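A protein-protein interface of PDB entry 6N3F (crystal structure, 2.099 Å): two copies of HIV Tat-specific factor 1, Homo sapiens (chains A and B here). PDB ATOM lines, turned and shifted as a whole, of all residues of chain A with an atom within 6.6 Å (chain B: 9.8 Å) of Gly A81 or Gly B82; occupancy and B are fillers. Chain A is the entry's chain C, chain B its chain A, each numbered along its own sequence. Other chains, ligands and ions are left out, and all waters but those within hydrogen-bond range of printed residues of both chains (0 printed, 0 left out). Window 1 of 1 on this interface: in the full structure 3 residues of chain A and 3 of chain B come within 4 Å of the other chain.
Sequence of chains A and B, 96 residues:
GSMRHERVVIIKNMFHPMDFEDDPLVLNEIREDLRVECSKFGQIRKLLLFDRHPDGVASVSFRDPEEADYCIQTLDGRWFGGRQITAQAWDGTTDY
The backbone carbonyl oxygen of Gly B81 is in hydrogen-bond range of the guanidinium group of Arg A83 (3.3 Å). The backbone NH of Gly B82 lies within hydrogen-bond range of the backbone carbonyl oxygen of Gly A81, 3.0 Å away.
OD2 of Asp A19 is in salt-bridge range of NH1 of Arg A83 (2.9 Å).
CB of Trp B79 touches C of Gly A81, 3.7 Å away. Trp B79 touches Gly A82. Gly A82 touches Gly B81 (O to N, 3.6 Å). Gly B82 touches Arg A83.
Gly A81 touches just these residues of chain B: Trp B79 and Gly B82. Gly B82 touches two residues of chain A. Arg A83 touches just these residues of chain B: Gly B81 (3.3 Å) and Gly B82 (3.3 Å). Printed residues of chain A within 4 Å of Gly B81: Gly A82 and Arg A83. Printed residues of chain A within 4 Å of Trp B79: Gly A81 and Gly A82. Trp A79 touches none of the printed residues of chain B. Phe B80 touches none of the printed residues of chain A. The nearest residue of chain A that does not touch Gly B82 is Asp A19 (4.7 Å).
Among the printed residues, 6 pairs touch across the chains. Among the printed residues, no Asp or Glu carboxylate lies within 4 Å of a Lys or Arg side-chain nitrogen of the other chain.
Gly A81 touches Trp B79, but with the chains exchanged Trp A79 does not touch Gly B81 (6.7 Å). Gly A81 touches Gly B82, and with the chains exchanged Gly A82 touches Gly B81. Gly A82 touches Trp B79, but with the chains exchanged Trp A79 does not touch Gly B82 (8.4 Å). Arg A83 touches Gly B81, but with the chains exchanged Gly A81 does not touch Arg B83 (4.4 Å). Of the 6 pairs that touch across the chains among the printed residues, 2 have their exchanged pair printed and touching as well.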
ATOM      1  N   MET A  14      -3.375  14.007   2.297  1.00  0.00           N
ATOM      2  CA  MET A  14      -4.139  14.917   1.459  1.00  0.00           C
ATOM      3  C   MET A  14      -3.846  16.380   1.778  1.00  0.00           C
ATOM      4  O   MET A  14      -4.107  17.242   0.943  1.00  0.00           O
ATOM      5  CB  MET A  14      -5.621  14.626   1.625  1.00  0.00           C
ATOM      6  CG  MET A  14      -6.558  15.470   0.813  1.00  0.00           C
ATOM      7  SD  MET A  14      -8.197  15.338   1.615  1.00  0.00           S
ATOM      8  CE  MET A  14      -9.136  16.371   0.529  1.00  0.00           C
ATOM      9  N   ASP A  19      -1.195  23.887   6.214  1.00  0.00           N
ATOM     10  CA  ASP A  19      -1.842  24.460   5.039  1.00  0.00           C
ATOM     11  C   ASP A  19      -2.931  25.474   5.394  1.00  0.00           C
ATOM     12  O   ASP A  19      -3.331  26.255   4.522  1.00  0.00           O
ATOM     13  CB  ASP A  19      -2.508  23.383   4.169  1.00  0.00           C
ATOM     14  CG  ASP A  19      -1.521  22.370   3.597  1.00  0.00           C
ATOM     15  OD1 ASP A  19      -0.295  22.597   3.631  1.00  0.00           O
ATOM     16  OD2 ASP A  19      -1.985  21.321   3.119  1.00  0.00           O
ATOM     17  N   TRP A  79      -2.566  12.043  -7.091  1.00  0.00           N
ATOM     18  CA  TRP A  79      -1.886  13.249  -6.643  1.00  0.00           C
ATOM     19  C   TRP A  79      -2.908  14.360  -6.421  1.00  0.00           C
ATOM     20  O   TRP A  79      -3.754  14.597  -7.278  1.00  0.00           O
ATOM     21  CB  TRP A  79      -0.823  13.658  -7.662  1.00  0.00           C
ATOM     22  CG  TRP A  79       0.414  12.764  -7.654  1.00  0.00           C
ATOM     23  CD1 TRP A  79       0.574  11.589  -8.322  1.00  0.00           C
ATOM     24  CD2 TRP A  79       1.659  13.002  -6.956  1.00  0.00           C
ATOM     25  NE1 TRP A  79       1.830  11.069  -8.081  1.00  0.00           N
ATOM     26  CE2 TRP A  79       2.515  11.918  -7.250  1.00  0.00           C
ATOM     27  CE3 TRP A  79       2.127  14.019  -6.110  1.00  0.00           C
ATOM     28  CZ2 TRP A  79       3.816  11.823  -6.729  1.00  0.00           C
ATOM     29  CZ3 TRP A  79       3.415  13.918  -5.584  1.00  0.00           C
ATOM     30  CH2 TRP A  79       4.246  12.835  -5.907  1.00  0.00           C
ATOM     31  N   PHE A  80      -2.830  15.026  -5.260  1.00  0.00           N
ATOM     32  CA  PHE A  80      -3.775  16.067  -4.851  1.00  0.00           C
ATOM     33  C   PHE A  80      -2.974  17.253  -4.312  1.00  0.00           C
ATOM     34  O   PHE A  80      -2.312  17.160  -3.266  1.00  0.00           O
ATOM     35  CB  PHE A  80      -4.773  15.538  -3.799  1.00  0.00           C
ATOM     36  CG  PHE A  80      -5.763  16.577  -3.294  1.00  0.00           C
ATOM     37  CD1 PHE A  80      -6.986  16.781  -3.938  1.00  0.00           C
ATOM     38  CD2 PHE A  80      -5.472  17.352  -2.175  1.00  0.00           C
ATOM     39  CE1 PHE A  80      -7.896  17.754  -3.463  1.00  0.00           C
ATOM     40  CE2 PHE A  80      -6.380  18.320  -1.706  1.00  0.00           C
ATOM     41  CZ  PHE A  80      -7.575  18.519  -2.340  1.00  0.00           C
ATOM     42  N   GLY A  81      -3.040  18.372  -5.018  1.00  0.00           N
ATOM     43  CA  GLY A  81      -2.239  19.526  -4.642  1.00  0.00           C
ATOM     44  C   GLY A  81      -0.761  19.243  -4.493  1.00  0.00           C
ATOM     45  O   GLY A  81      -0.119  19.805  -3.601  1.00  0.00           O
ATOM     46  N   GLY A  82      -0.199  18.383  -5.341  1.00  0.00           N
ATOM     47  CA  GLY A  82       1.222  18.092  -5.287  1.00  0.00           C
ATOM     48  C   GLY A  82       1.646  17.070  -4.252  1.00  0.00           C
ATOM     49  O   GLY A  82       2.852  16.847  -4.087  1.00  0.00           O
ATOM     50  N   ARG A  83       0.696  16.436  -3.562  1.00  0.00           N
ATOM     51  CA  ARG A  83       0.961  15.373  -2.602  1.00  0.00           C
ATOM     52  C   ARG A  83       0.350  14.064  -3.104  1.00  0.00           C
ATOM     53  O   ARG A  83      -0.796  14.038  -3.566  1.00  0.00           O
ATOM     54  CB  ARG A  83       0.378  15.736  -1.225  1.00  0.00           C
ATOM     55  CG  ARG A  83       1.101  16.860  -0.467  1.00  0.00           C
ATOM     56  CD  ARG A  83       0.626  17.001   1.043  1.00  0.00           C
ATOM     57  NE  ARG A  83       1.277  18.137   1.737  1.00  0.00           N
ATOM     58  CZ  ARG A  83       0.745  19.360   1.867  1.00  0.00           C
ATOM     59  NH1 ARG A  83      -0.467  19.631   1.364  1.00  0.00           N
ATOM     60  NH2 ARG A  83       1.414  20.333   2.508  1.00  0.00           N
ATOM     61  N   ASN B  13       6.866  30.265  -3.670  1.00  0.00           N
ATOM     62  CA  ASN B  13       6.054  29.272  -2.973  1.00  0.00           C
ATOM     63  C   ASN B  13       6.587  27.866  -3.177  1.00  0.00           C
ATOM     64  O   ASN B  13       5.823  26.906  -3.211  1.00  0.00           O
ATOM     65  CB  ASN B  13       4.588  29.338  -3.387  1.00  0.00           C
ATOM     66  CG  ASN B  13       3.905  30.563  -2.866  1.00  0.00           C
ATOM     67  OD1 ASN B  13       4.343  31.167  -1.865  1.00  0.00           O
ATOM     68  ND2 ASN B  13       2.820  30.950  -3.532  1.00  0.00           N
ATOM     69  N   MET B  14       7.894  27.740  -3.306  1.00  0.00           N
ATOM     70  CA  MET B  14       8.508  26.460  -3.551  1.00  0.00           C
ATOM     71  C   MET B  14       8.872  25.721  -2.276  1.00  0.00           C
ATOM     72  O   MET B  14       9.146  24.521  -2.338  1.00  0.00           O
ATOM     73  CB  MET B  14       9.768  26.626  -4.373  1.00  0.00           C
ATOM     74  CG  MET B  14      10.354  25.308  -4.805  1.00  0.00           C
ATOM     75  SD  MET B  14      11.586  25.585  -6.059  1.00  0.00           S
ATOM     76  CE  MET B  14      12.741  26.459  -5.034  1.00  0.00           C
ATOM     77  N   PHE B  15       8.888  26.409  -1.144  1.00  0.00           N
ATOM     78  CA  PHE B  15       9.259  25.826   0.143  1.00  0.00           C
ATOM     79  C   PHE B  15       8.825  26.831   1.202  1.00  0.00           C
ATOM     80  O   PHE B  15       8.414  27.943   0.882  1.00  0.00           O
ATOM     81  CB  PHE B  15      10.770  25.545   0.236  1.00  0.00           C
ATOM     82  CG  PHE B  15      11.630  26.777   0.002  1.00  0.00           C
ATOM     83  CD1 PHE B  15      11.957  27.620   1.052  1.00  0.00           C
ATOM     84  CD2 PHE B  15      12.078  27.099  -1.277  1.00  0.00           C
ATOM     85  CE1 PHE B  15      12.735  28.764   0.842  1.00  0.00           C
ATOM     86  CE2 PHE B  15      12.846  28.227  -1.500  1.00  0.00           C
ATOM     87  CZ  PHE B  15      13.181  29.058  -0.435  1.00  0.00           C
ATOM     88  N   ASP B  19      10.830  24.140   6.501  1.00  0.00           N
ATOM     89  CA  ASP B  19      11.101  22.853   5.869  1.00  0.00           C
ATOM     90  C   ASP B  19      12.524  22.378   6.146  1.00  0.00           C
ATOM     91  O   ASP B  19      12.784  21.169   6.153  1.00  0.00           O
ATOM     92  CB  ASP B  19      10.867  22.959   4.347  1.00  0.00           C
ATOM     93  CG  ASP B  19       9.395  23.235   3.984  1.00  0.00           C
ATOM     94  OD1 ASP B  19       8.528  23.117   4.872  1.00  0.00           O
ATOM     95  OD2 ASP B  19       9.083  23.555   2.812  1.00  0.00           O
ATOM     96  N   GLY B  77       2.038  27.892 -11.860  1.00  0.00           N
ATOM     97  CA  GLY B  77       0.798  27.227 -11.515  1.00  0.00           C
ATOM     98  C   GLY B  77       0.925  25.749 -11.213  1.00  0.00           C
ATOM     99  O   GLY B  77      -0.090  25.096 -10.940  1.00  0.00           O
ATOM    100  N   ARG B  78       2.133  25.205 -11.248  1.00  0.00           N
ATOM    101  CA  ARG B  78       2.374  23.819 -10.902  1.00  0.00           C
ATOM    102  C   ARG B  78       2.237  23.600  -9.394  1.00  0.00           C
ATOM    103  O   ARG B  78       2.714  24.396  -8.583  1.00  0.00           O
ATOM    104  CB  ARG B  78       3.763  23.430 -11.388  1.00  0.00           C
ATOM    105  CG  ARG B  78       4.216  22.004 -11.106  1.00  0.00           C
ATOM    106  CD  ARG B  78       5.439  21.640 -11.952  1.00  0.00           C
ATOM    107  NE  ARG B  78       5.073  21.384 -13.344  1.00  0.00           N
ATOM    108  CZ  ARG B  78       5.922  20.964 -14.278  1.00  0.00           C
ATOM    109  NH1 ARG B  78       7.200  20.761 -13.971  1.00  0.00           N
ATOM    110  NH2 ARG B  78       5.492  20.745 -15.520  1.00  0.00           N
ATOM    111  N   TRP B  79       1.574  22.508  -9.018  1.00  0.00           N
ATOM    112  CA  TRP B  79       1.399  22.180  -7.609  1.00  0.00           C
ATOM    113  C   TRP B  79       2.625  21.472  -7.070  1.00  0.00           C
ATOM    114  O   TRP B  79       3.273  20.675  -7.759  1.00  0.00           O
ATOM    115  CB  TRP B  79       0.169  21.303  -7.374  1.00  0.00           C
ATOM    116  CG  TRP B  79      -1.099  22.070  -7.482  1.00  0.00           C
ATOM    117  CD1 TRP B  79      -1.884  22.196  -8.596  1.00  0.00           C
ATOM    118  CD2 TRP B  79      -1.739  22.839  -6.451  1.00  0.00           C
ATOM    119  NE1 TRP B  79      -2.980  22.977  -8.320  1.00  0.00           N
ATOM    120  CE2 TRP B  79      -2.918  23.388  -7.014  1.00  0.00           C
ATOM    121  CE3 TRP B  79      -1.447  23.096  -5.096  1.00  0.00           C
ATOM    122  CZ2 TRP B  79      -3.793  24.198  -6.287  1.00  0.00           C
ATOM    123  CZ3 TRP B  79      -2.323  23.903  -4.366  1.00  0.00           C
ATOM    124  CH2 TRP B  79      -3.485  24.446  -4.968  1.00  0.00           C
ATOM    125  N   PHE B  80       2.931  21.770  -5.812  1.00  0.00           N
ATOM    126  CA  PHE B  80       4.152  21.274  -5.197  1.00  0.00           C
ATOM    127  C   PHE B  80       3.984  21.304  -3.677  1.00  0.00           C
ATOM    128  O   PHE B  80       3.906  22.381  -3.078  1.00  0.00           O
ATOM    129  CB  PHE B  80       5.333  22.107  -5.675  1.00  0.00           C
ATOM    130  CG  PHE B  80       6.626  21.492  -5.371  1.00  0.00           C
ATOM    131  CD1 PHE B  80       6.879  20.200  -5.764  1.00  0.00           C
ATOM    132  CD2 PHE B  80       7.582  22.181  -4.654  1.00  0.00           C
ATOM    133  CE1 PHE B  80       8.066  19.600  -5.462  1.00  0.00           C
ATOM    134  CE2 PHE B  80       8.787  21.599  -4.355  1.00  0.00           C
ATOM    135  CZ  PHE B  80       9.034  20.302  -4.756  1.00  0.00           C
ATOM    136  N   GLY B  81       3.869  20.117  -3.069  1.00  0.00           N
ATOM    137  CA  GLY B  81       3.743  19.998  -1.635  1.00  0.00           C
ATOM    138  C   GLY B  81       2.774  20.968  -0.988  1.00  0.00           C
ATOM    139  O   GLY B  81       3.118  21.657  -0.022  1.00  0.00           O
ATOM    140  N   GLY B  82       1.561  21.043  -1.512  1.00  0.00           N
ATOM    141  CA  GLY B  82       0.513  21.830  -0.912  1.00  0.00           C
ATOM    142  C   GLY B  82       0.303  23.205  -1.524  1.00  0.00           C
ATOM    143  O   GLY B  82      -0.791  23.760  -1.372  1.00  0.00           O
ATOM    144  N   ARG B  83       1.312  23.776  -2.197  1.00  0.00           N
ATOM    145  CA  ARG B  83       1.231  25.121  -2.757  1.00  0.00           C
ATOM    146  C   ARG B  83       1.357  25.077  -4.270  1.00  0.00           C
ATOM    147  O   ARG B  83       2.047  24.218  -4.823  1.00  0.00           O
ATOM    148  CB  ARG B  83       2.341  26.032  -2.221  1.00  0.00           C
ATOM    149  CG  ARG B  83       2.565  25.945  -0.703  1.00  0.00           C
ATOM    150  CD  ARG B  83       3.608  26.950  -0.254  1.00  0.00           C
ATOM    151  NE  ARG B  83       3.985  26.709   1.132  1.00  0.00           N
ATOM    152  CZ  ARG B  83       4.805  25.737   1.515  1.00  0.00           C
ATOM    153  NH1 ARG B  83       5.338  24.919   0.617  1.00  0.00           N
ATOM    154  NH2 ARG B  83       5.092  25.587   2.790  1.00  0.00           N
ATOM    155  N   GLN B  84       0.676  26.016  -4.928  1.00  0.00           N
ATOM    156  CA  GLN B  84       0.964  26.364  -6.311  1.00  0.00           C
ATOM    157  C   GLN B  84       2.199  27.253  -6.335  1.00  0.00           C
ATOM    158  O   GLN B  84       2.225  28.322  -5.702  1.00  0.00           O
ATOM    159  CB  GLN B  84      -0.207  27.102  -6.951  1.00  0.00           C
ATOM    160  CG  GLN B  84      -1.203  26.235  -7.607  1.00  0.00           C
ATOM    161  CD  GLN B  84      -2.267  27.039  -8.325  1.00  0.00           C
ATOM    162  OE1 GLN B  84      -2.802  28.006  -7.779  1.00  0.00           O
ATOM    163  NE2 GLN B  84      -2.580  26.645  -9.558  1.00  0.00           N
ATOM    164  N   ILE B  85       3.214  26.824  -7.029  1.00  0.00           N
ATOM    165  CA  ILE B  85       4.335  27.723  -7.258  1.00  0.00           C
ATOM    166  C   ILE B  85       3.951  28.728  -8.334  1.00  0.00           C
ATOM    167  O   ILE B  85       3.101  28.470  -9.191  1.00  0.00           O
ATOM    168  CB  ILE B  85       5.609  26.942  -7.614  1.00  0.00           C
ATOM    169  CG1 ILE B  85       5.502  26.337  -8.997  1.00  0.00           C
ATOM    170  CG2 ILE B  85       5.862  25.825  -6.571  1.00  0.00           C
ATOM    171  CD1 ILE B  85       6.768  25.674  -9.414  1.00  0.00           C
